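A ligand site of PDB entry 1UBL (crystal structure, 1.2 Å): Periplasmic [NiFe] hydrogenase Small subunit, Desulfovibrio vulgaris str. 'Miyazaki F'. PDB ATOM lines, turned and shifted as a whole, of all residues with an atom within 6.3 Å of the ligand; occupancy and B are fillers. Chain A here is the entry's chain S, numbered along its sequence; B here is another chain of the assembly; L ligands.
The backbone carbonyl oxygen of Gly 149 sits close to a sulfur (S1) of the ligand (3.6 Å).
N of Pro 151 sits close to S2 of the ligand, 3.6 Å away.
Glu 16 touches the ligand.
Gly 19 touches the ligand.
Glu 75 touches the ligand.
Gly 112 touches the ligand.
CG1 of Val 120 touches S4 of the ligand, 3.9 Å away.
Arg 61 of chain B touches the ligand.
Within 4 Å of the ligand: Glu 16, Cys 17, Gly 19, Cys 20, Glu 75, Gly 112, Thr 113, Cys 114, Val 120, Gly 149, Cys 150, Pro 151, Arg 61 of chain B and His 217 of chain B.
The side-chain sulfur (SG) of Cys 20 is bound to an iron atom (FE4) of the ligand, 2.2 Å away.
The backbone NH (N) of Cys 114 sits close to a sulfur (S1) of the ligand, at 3.5 Å.
An iron atom (FE2) of the ligand is bound by the side-chain sulfur (SG) of Cys 114 (2.3 Å).
The backbone NH (N) of Cys 17 sits close to a sulfur (S3) of the ligand, 3.5 Å away.
FE1 of the ligand is bound by SG of Cys 17 (2.3 Å).
SG of Cys 150 binds FE3 of the ligand (2.3 Å).
A sulfur (S1) of the ligand sits close to the backbone NH (N) of Thr 113, at 3.4 Å.
A sulfur (S2) of the ligand lies close to a ring nitrogen (ND1) of His 217 of chain B (3.7 Å).
The side-chain sulfur (SG) of Cys 20 lies close to the backbone carbonyl oxygen (O) of Tyr 111, at 3.7 Å.
NE2 of Gln 121 lies close to SG of Cys 114, at 3.3 Å.
The backbone carbonyl oxygen (O) of Cys 17 is in hydrogen-bond range of the backbone NH (N) of Gly 64 of chain B, at 2.8 Å.
OG1 of Thr 113 sits at hydrogen-bond distance from N of Gly 149, 2.8 Å away.
A ring nitrogen (ND1) of His 217 of chain B lies within hydrogen-bond range of the guanidinium group (NE) of Arg 61 of chain B (3.4 Å).
NH1 of Arg 41 of chain B is in hydrogen-bond range of O of Arg 61 of chain B (2.8 Å).
The side-chain carboxylate (OE1) of Glu 16 is in hydrogen-bond range of the side-chain hydroxyl (OG1) of Thr 18 (2.6 Å).
The side-chain carboxylate (OE1) of Glu 75 sits close to the backbone NH (N) of Thr 18 (3.4 Å).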
ATOM      1  N   ALA A  15     -13.102  17.429 -24.781  1.00  0.00           N
ATOM      2  CA  ALA A  15     -12.930  18.844 -25.177  1.00  0.00           C
ATOM      3  C   ALA A  15     -12.199  19.520 -24.035  1.00  0.00           C
ATOM      4  O   ALA A  15     -12.794  19.850 -23.005  1.00  0.00           O
ATOM      5  CB  ALA A  15     -14.278  19.508 -25.475  1.00  0.00           C
ATOM      6  N   GLU A  16     -10.893  19.679 -24.230  1.00  0.00           N
ATOM      7  CA  GLU A  16     -10.015  20.091 -23.136  1.00  0.00           C
ATOM      8  C   GLU A  16      -8.846  20.889 -23.702  1.00  0.00           C
ATOM      9  O   GLU A  16      -8.608  20.873 -24.913  1.00  0.00           O
ATOM     10  CB  GLU A  16      -9.508  18.882 -22.347  1.00  0.00           C
ATOM     11  CG  GLU A  16      -9.041  17.677 -23.175  1.00  0.00           C
ATOM     12  CD  GLU A  16      -7.660  17.764 -23.721  1.00  0.00           C
ATOM     13  OE1 GLU A  16      -6.755  18.229 -23.026  1.00  0.00           O
ATOM     14  OE2 GLU A  16      -7.465  17.310 -24.887  1.00  0.00           O
ATOM     15  N   CYS A  17      -8.153  21.601 -22.811  1.00  0.00           N
ATOM     16  CA  CYS A  17      -7.032  22.411 -23.172  1.00  0.00           C
ATOM     17  C   CYS A  17      -5.707  21.758 -22.757  1.00  0.00           C
ATOM     18  O   CYS A  17      -4.645  22.331 -23.028  1.00  0.00           O
ATOM     19  CB  CYS A  17      -7.115  23.805 -22.527  1.00  0.00           C
ATOM     20  SG  CYS A  17      -6.645  23.913 -20.777  1.00  0.00           S
ATOM     21  N   THR A  18      -5.753  20.629 -22.057  1.00  0.00           N
ATOM     22  CA  THR A  18      -4.605  19.870 -21.536  1.00  0.00           C
ATOM     23  C   THR A  18      -3.993  20.524 -20.314  1.00  0.00           C
ATOM     24  O   THR A  18      -3.029  19.971 -19.703  1.00  0.00           O
ATOM     25  CB  THR A  18      -3.631  19.518 -22.685  1.00  0.00           C
ATOM     26  OG1 THR A  18      -4.412  19.037 -23.812  1.00  0.00           O
ATOM     27  CG2 THR A  18      -2.591  18.488 -22.306  1.00  0.00           C
ATOM     28  N   GLY A  19      -4.568  21.622 -19.829  1.00  0.00           N
ATOM     29  CA  GLY A  19      -4.119  22.200 -18.539  1.00  0.00           C
ATOM     30  C   GLY A  19      -4.349  21.272 -17.396  1.00  0.00           C
ATOM     31  O   GLY A  19      -3.588  21.264 -16.425  1.00  0.00           O
ATOM     32  N   CYS A  20      -5.437  20.464 -17.432  1.00  0.00           N
ATOM     33  CA  CYS A  20      -5.620  19.513 -16.316  1.00  0.00           C
ATOM     34  C   CYS A  20      -4.540  18.445 -16.373  1.00  0.00           C
ATOM     35  O   CYS A  20      -3.957  18.111 -15.324  1.00  0.00           O
ATOM     36  CB  CYS A  20      -7.036  18.945 -16.409  1.00  0.00           C
ATOM     37  SG  CYS A  20      -8.308  20.103 -15.847  1.00  0.00           S
ATOM     38  N   SER A  21      -4.203  17.908 -17.549  1.00  0.00           N
ATOM     39  CA  SER A  21      -3.076  16.948 -17.625  1.00  0.00           C
ATOM     40  C   SER A  21      -1.789  17.562 -17.112  1.00  0.00           C
ATOM     41  O   SER A  21      -1.037  16.935 -16.374  1.00  0.00           O
ATOM     42  CB  SER A  21      -2.827  16.461 -19.056  1.00  0.00           C
ATOM     43  OG  SER A  21      -3.819  15.590 -19.511  1.00  0.00           O
ATOM     44  N   GLU A  75     -10.664  14.128 -18.517  1.00  0.00           N
ATOM     45  CA  GLU A  75     -10.398  15.552 -18.698  1.00  0.00           C
ATOM     46  C   GLU A  75     -11.197  16.058 -19.885  1.00  0.00           C
ATOM     47  O   GLU A  75     -11.221  15.431 -20.926  1.00  0.00           O
ATOM     48  CB  GLU A  75      -8.899  15.756 -18.931  1.00  0.00           C
ATOM     49  CG  GLU A  75      -8.430  17.174 -19.271  1.00  0.00           C
ATOM     50  CD  GLU A  75      -6.893  17.272 -19.345  1.00  0.00           C
ATOM     51  OE1 GLU A  75      -6.423  18.428 -19.557  1.00  0.00           O
ATOM     52  OE2 GLU A  75      -6.220  16.217 -19.187  1.00  0.00           O
ATOM     53  N   GLY A  76     -11.876  17.190 -19.713  1.00  0.00           N
ATOM     54  CA  GLY A  76     -12.600  17.818 -20.797  1.00  0.00           C
ATOM     55  C   GLY A  76     -14.113  17.538 -20.755  1.00  0.00           C
ATOM     56  O   GLY A  76     -14.582  16.529 -20.253  1.00  0.00           O
ATOM     57  N   GLY A  77     -14.849  18.493 -21.336  1.00  0.00           N
ATOM     58  CA  GLY A  77     -16.284  18.319 -21.491  1.00  0.00           C
ATOM     59  C   GLY A  77     -16.580  17.437 -22.722  1.00  0.00           C
ATOM     60  O   GLY A  77     -15.734  17.243 -23.598  1.00  0.00           O
ATOM     61  N   TYR A 111     -12.007  15.141 -13.828  1.00  0.00           N
ATOM     62  CA  TYR A 111     -10.906  15.993 -13.321  1.00  0.00           C
ATOM     63  C   TYR A 111     -10.924  17.289 -14.145  1.00  0.00           C
ATOM     64  O   TYR A 111     -10.721  17.277 -15.377  1.00  0.00           O
ATOM     65  CB  TYR A 111      -9.573  15.225 -13.432  1.00  0.00           C
ATOM     66  CG  TYR A 111      -8.417  16.040 -12.804  1.00  0.00           C
ATOM     67  CD1 TYR A 111      -8.447  16.377 -11.453  1.00  0.00           C
ATOM     68  CD2 TYR A 111      -7.353  16.429 -13.604  1.00  0.00           C
ATOM     69  CE1 TYR A 111      -7.412  17.103 -10.869  1.00  0.00           C
ATOM     70  CE2 TYR A 111      -6.322  17.185 -13.032  1.00  0.00           C
ATOM     71  CZ  TYR A 111      -6.349  17.522 -11.690  1.00  0.00           C
ATOM     72  OH  TYR A 111      -5.369  18.272 -11.091  1.00  0.00           O
ATOM     73  N   GLY A 112     -11.193  18.398 -13.415  1.00  0.00           N
ATOM     74  CA  GLY A 112     -11.251  19.746 -14.012  1.00  0.00           C
ATOM     75  C   GLY A 112     -12.701  20.166 -14.253  1.00  0.00           C
ATOM     76  O   GLY A 112     -13.581  19.343 -14.540  1.00  0.00           O
ATOM     77  N   THR A 113     -12.917  21.479 -14.145  1.00  0.00           N
ATOM     78  CA  THR A 113     -14.279  22.032 -14.321  1.00  0.00           C
ATOM     79  C   THR A 113     -14.898  21.670 -15.642  1.00  0.00           C
ATOM     80  O   THR A 113     -16.118  21.527 -15.735  1.00  0.00           O
ATOM     81  CB  THR A 113     -14.177  23.556 -14.124  1.00  0.00           C
ATOM     82  OG1 THR A 113     -13.854  23.692 -12.719  1.00  0.00           O
ATOM     83  CG2 THR A 113     -15.491  24.297 -14.443  1.00  0.00           C
ATOM     84  N   CYS A 114     -14.136  21.487 -16.730  1.00  0.00           N
ATOM     85  CA  CYS A 114     -14.728  21.042 -17.991  1.00  0.00           C
ATOM     86  C   CYS A 114     -15.362  19.640 -17.834  1.00  0.00           C
ATOM     87  O   CYS A 114     -16.519  19.464 -18.189  1.00  0.00           O
ATOM     88  CB  CYS A 114     -13.737  20.969 -19.149  1.00  0.00           C
ATOM     89  SG  CYS A 114     -13.035  22.600 -19.612  1.00  0.00           S
ATOM     90  N   ALA A 115     -14.589  18.682 -17.304  1.00  0.00           N
ATOM     91  CA  ALA A 115     -15.185  17.347 -17.148  1.00  0.00           C
ATOM     92  C   ALA A 115     -16.254  17.337 -16.074  1.00  0.00           C
ATOM     93  O   ALA A 115     -17.221  16.579 -16.148  1.00  0.00           O
ATOM     94  CB  ALA A 115     -14.069  16.351 -16.768  1.00  0.00           C
ATOM     95  N   GLY A 119     -17.491  23.396 -18.399  1.00  0.00           N
ATOM     96  CA  GLY A 119     -16.318  24.239 -18.569  1.00  0.00           C
ATOM     97  C   GLY A 119     -16.381  25.252 -19.684  1.00  0.00           C
ATOM     98  O   GLY A 119     -17.441  25.722 -20.134  1.00  0.00           O
ATOM     99  N   VAL A 120     -15.202  25.638 -20.200  1.00  0.00           N
ATOM    100  CA  VAL A 120     -15.095  26.853 -21.007  1.00  0.00           C
ATOM    101  C   VAL A 120     -15.897  26.678 -22.291  1.00  0.00           C
ATOM    102  O   VAL A 120     -16.549  27.633 -22.733  1.00  0.00           O
ATOM    103  CB  VAL A 120     -13.613  27.218 -21.205  1.00  0.00           C
ATOM    104  CG1 VAL A 120     -12.865  26.199 -22.078  1.00  0.00           C
ATOM    105  CG2 VAL A 120     -13.485  28.619 -21.780  1.00  0.00           C
ATOM    106  N   GLN A 121     -15.870  25.529 -22.955  1.00  0.00           N
ATOM    107  CA  GLN A 121     -16.600  25.357 -24.228  1.00  0.00           C
ATOM    108  C   GLN A 121     -18.099  25.254 -23.966  1.00  0.00           C
ATOM    109  O   GLN A 121     -18.851  25.432 -24.948  1.00  0.00           O
ATOM    110  CB  GLN A 121     -16.085  24.137 -25.010  1.00  0.00           C
ATOM    111  CG  GLN A 121     -16.142  22.818 -24.259  1.00  0.00           C
ATOM    112  CD  GLN A 121     -14.899  22.609 -23.426  1.00  0.00           C
ATOM    113  OE1 GLN A 121     -13.795  22.859 -23.868  1.00  0.00           O
ATOM    114  NE2 GLN A 121     -15.033  22.164 -22.177  1.00  0.00           N
ATOM    115  N   GLY A 149     -12.031  22.805 -10.718  1.00  0.00           N
ATOM    116  CA  GLY A 149     -10.988  23.809 -10.791  1.00  0.00           C
ATOM    117  C   GLY A 149     -10.516  23.846 -12.248  1.00  0.00           C
ATOM    118  O   GLY A 149     -10.673  22.895 -13.010  1.00  0.00           O
ATOM    119  N   CYS A 150      -9.838  24.976 -12.607  1.00  0.00           N
ATOM    120  CA  CYS A 150      -9.477  25.182 -14.026  1.00  0.00           C
ATOM    121  C   CYS A 150      -8.026  25.640 -14.161  1.00  0.00           C
ATOM    122  O   CYS A 150      -7.728  26.802 -14.496  1.00  0.00           O
ATOM    123  CB  CYS A 150     -10.496  26.192 -14.627  1.00  0.00           C
ATOM    124  SG  CYS A 150     -10.457  26.311 -16.440  1.00  0.00           S
ATOM    125  N   PRO A 151      -7.070  24.730 -13.922  1.00  0.00           N
ATOM    126  CA  PRO A 151      -7.264  23.336 -13.513  1.00  0.00           C
ATOM    127  C   PRO A 151      -7.351  23.205 -12.005  1.00  0.00           C
ATOM    128  O   PRO A 151      -7.047  24.133 -11.220  1.00  0.00           O
ATOM    129  CB  PRO A 151      -5.998  22.640 -14.051  1.00  0.00           C
ATOM    130  CG  PRO A 151      -4.925  23.729 -13.878  1.00  0.00           C
ATOM    131  CD  PRO A 151      -5.642  25.050 -14.198  1.00  0.00           C
ATOM    132  N   PRO A 152      -7.758  22.040 -11.514  1.00  0.00           N
ATOM    133  CA  PRO A 152      -7.776  21.773 -10.068  1.00  0.00           C
ATOM    134  C   PRO A 152      -6.372  21.744  -9.513  1.00  0.00           C
ATOM    135  O   PRO A 152      -5.367  21.645 -10.229  1.00  0.00           O
ATOM    136  CB  PRO A 152      -8.400  20.350  -9.950  1.00  0.00           C
ATOM    137  CG  PRO A 152      -9.090  20.166 -11.295  1.00  0.00           C
ATOM    138  CD  PRO A 152      -8.168  20.851 -12.306  1.00  0.00           C
ATOM    139  N   TRP A 258     -17.936  30.543 -15.978  1.00  0.00           N
ATOM    140  CA  TRP A 258     -17.696  31.459 -17.086  1.00  0.00           C
ATOM    141  C   TRP A 258     -18.865  32.438 -17.325  1.00  0.00           C
ATOM    142  O   TRP A 258     -18.633  33.557 -17.772  1.00  0.00           O
ATOM    143  CB  TRP A 258     -17.476  30.643 -18.376  1.00  0.00           C
ATOM    144  CG  TRP A 258     -16.263  29.732 -18.230  1.00  0.00           C
ATOM    145  CD1 TRP A 258     -16.239  28.382 -18.017  1.00  0.00           C
ATOM    146  CD2 TRP A 258     -14.912  30.167 -18.279  1.00  0.00           C
ATOM    147  NE1 TRP A 258     -14.929  27.965 -17.942  1.00  0.00           N
ATOM    148  CE2 TRP A 258     -14.087  29.048 -18.086  1.00  0.00           C
ATOM    149  CE3 TRP A 258     -14.285  31.429 -18.457  1.00  0.00           C
ATOM    150  CZ2 TRP A 258     -12.672  29.105 -18.081  1.00  0.00           C
ATOM    151  CZ3 TRP A 258     -12.906  31.469 -18.441  1.00  0.00           C
ATOM    152  CH2 TRP A 258     -12.080  30.360 -18.248  1.00  0.00           C
ATOM    153  N   ARG B  41     -13.930  23.773 -30.273  1.00  0.00           N
ATOM    154  CA  ARG B  41     -14.574  24.316 -29.083  1.00  0.00           C
ATOM    155  C   ARG B  41     -15.294  25.627 -29.362  1.00  0.00           C
ATOM    156  O   ARG B  41     -16.405  25.848 -28.782  1.00  0.00           O
ATOM    157  CB  ARG B  41     -13.552  24.494 -27.943  1.00  0.00           C
ATOM    158  CG  ARG B  41     -13.084  23.181 -27.342  1.00  0.00           C
ATOM    159  CD  ARG B  41     -11.952  23.230 -26.335  1.00  0.00           C
ATOM    160  NE  ARG B  41     -10.783  23.799 -26.971  1.00  0.00           N
ATOM    161  CZ  ARG B  41      -9.861  24.524 -26.358  1.00  0.00           C
ATOM    162  NH1 ARG B  41      -9.822  24.725 -25.037  1.00  0.00           N
ATOM    163  NH2 ARG B  41      -8.892  25.061 -27.145  1.00  0.00           N
ATOM    164  N   ARG B  61      -7.537  29.523 -21.632  1.00  0.00           N
ATOM    165  CA  ARG B  61      -8.009  28.150 -21.731  1.00  0.00           C
ATOM    166  C   ARG B  61      -8.067  27.641 -23.158  1.00  0.00           C
ATOM    167  O   ARG B  61      -8.505  26.527 -23.364  1.00  0.00           O
ATOM    168  CB  ARG B  61      -9.362  27.989 -21.019  1.00  0.00           C
ATOM    169  CG  ARG B  61      -9.317  27.916 -19.515  1.00  0.00           C
ATOM    170  CD  ARG B  61      -8.718  29.141 -18.857  1.00  0.00           C
ATOM    171  NE  ARG B  61      -8.730  28.943 -17.378  1.00  0.00           N
ATOM    172  CZ  ARG B  61      -8.327  29.861 -16.502  1.00  0.00           C
ATOM    173  NH1 ARG B  61      -8.032  31.095 -16.912  1.00  0.00           N
ATOM    174  NH2 ARG B  61      -8.278  29.480 -15.253  1.00  0.00           N
ATOM    175  N   GLY B  64      -3.459  24.716 -22.120  1.00  0.00           N
ATOM    176  CA  GLY B  64      -2.749  24.578 -20.838  1.00  0.00           C
ATOM    177  C   GLY B  64      -1.328  24.074 -20.991  1.00  0.00           C
ATOM    178  O   GLY B  64      -0.643  24.032 -19.947  1.00  0.00           O
ATOM    179  N   PRO B 216      -0.635  25.202 -13.928  1.00  0.00           N
ATOM    180  CA  PRO B 216      -1.075  25.958 -15.119  1.00  0.00           C
ATOM    181  C   PRO B 216      -2.041  27.073 -14.832  1.00  0.00           C
ATOM    182  O   PRO B 216      -2.742  27.141 -13.808  1.00  0.00           O
ATOM    183  CB  PRO B 216      -1.806  24.878 -15.995  1.00  0.00           C
ATOM    184  CG  PRO B 216      -1.273  23.550 -15.478  1.00  0.00           C
ATOM    185  CD  PRO B 216      -1.107  23.789 -14.006  1.00  0.00           C
ATOM    186  N   HIS B 217      -2.136  27.967 -15.840  1.00  0.00           N
ATOM    187  CA  HIS B 217      -3.082  29.065 -16.016  1.00  0.00           C
ATOM    188  C   HIS B 217      -2.821  30.144 -14.964  1.00  0.00           C
ATOM    189  O   HIS B 217      -3.375  30.229 -13.866  1.00  0.00           O
ATOM    190  CB  HIS B 217      -4.553  28.581 -16.000  1.00  0.00           C
ATOM    191  CG  HIS B 217      -4.876  27.792 -17.251  1.00  0.00           C
ATOM    192  ND1 HIS B 217      -5.918  26.952 -17.491  1.00  0.00           N
ATOM    193  CD2 HIS B 217      -4.131  27.891 -18.410  1.00  0.00           C
ATOM    194  CE1 HIS B 217      -5.810  26.527 -18.777  1.00  0.00           C
ATOM    195  NE2 HIS B 217      -4.725  27.091 -19.343  1.00  0.00           N
HETATM  196 FE1  LIG L   1      -8.400  23.318 -19.468  1.00  0.00          FE
HETATM  197 FE2  LIG L   1     -10.886  22.564 -18.891  1.00  0.00          FE
HETATM  198 FE3  LIG L   1      -9.702  24.370 -17.372  1.00  0.00          FE
HETATM  199 FE4  LIG L   1      -8.828  21.762 -17.271  1.00  0.00          FE
HETATM  200  S1  LIG L   1     -10.845  22.522 -16.576  1.00  0.00           S
HETATM  201  S2  LIG L   1      -7.567  23.691 -17.335  1.00  0.00           S
HETATM  202  S3  LIG L   1      -9.217  21.131 -19.500  1.00  0.00           S
HETATM  203  S4  LIG L   1     -10.213  24.613 -19.659  1.00  0.00           S
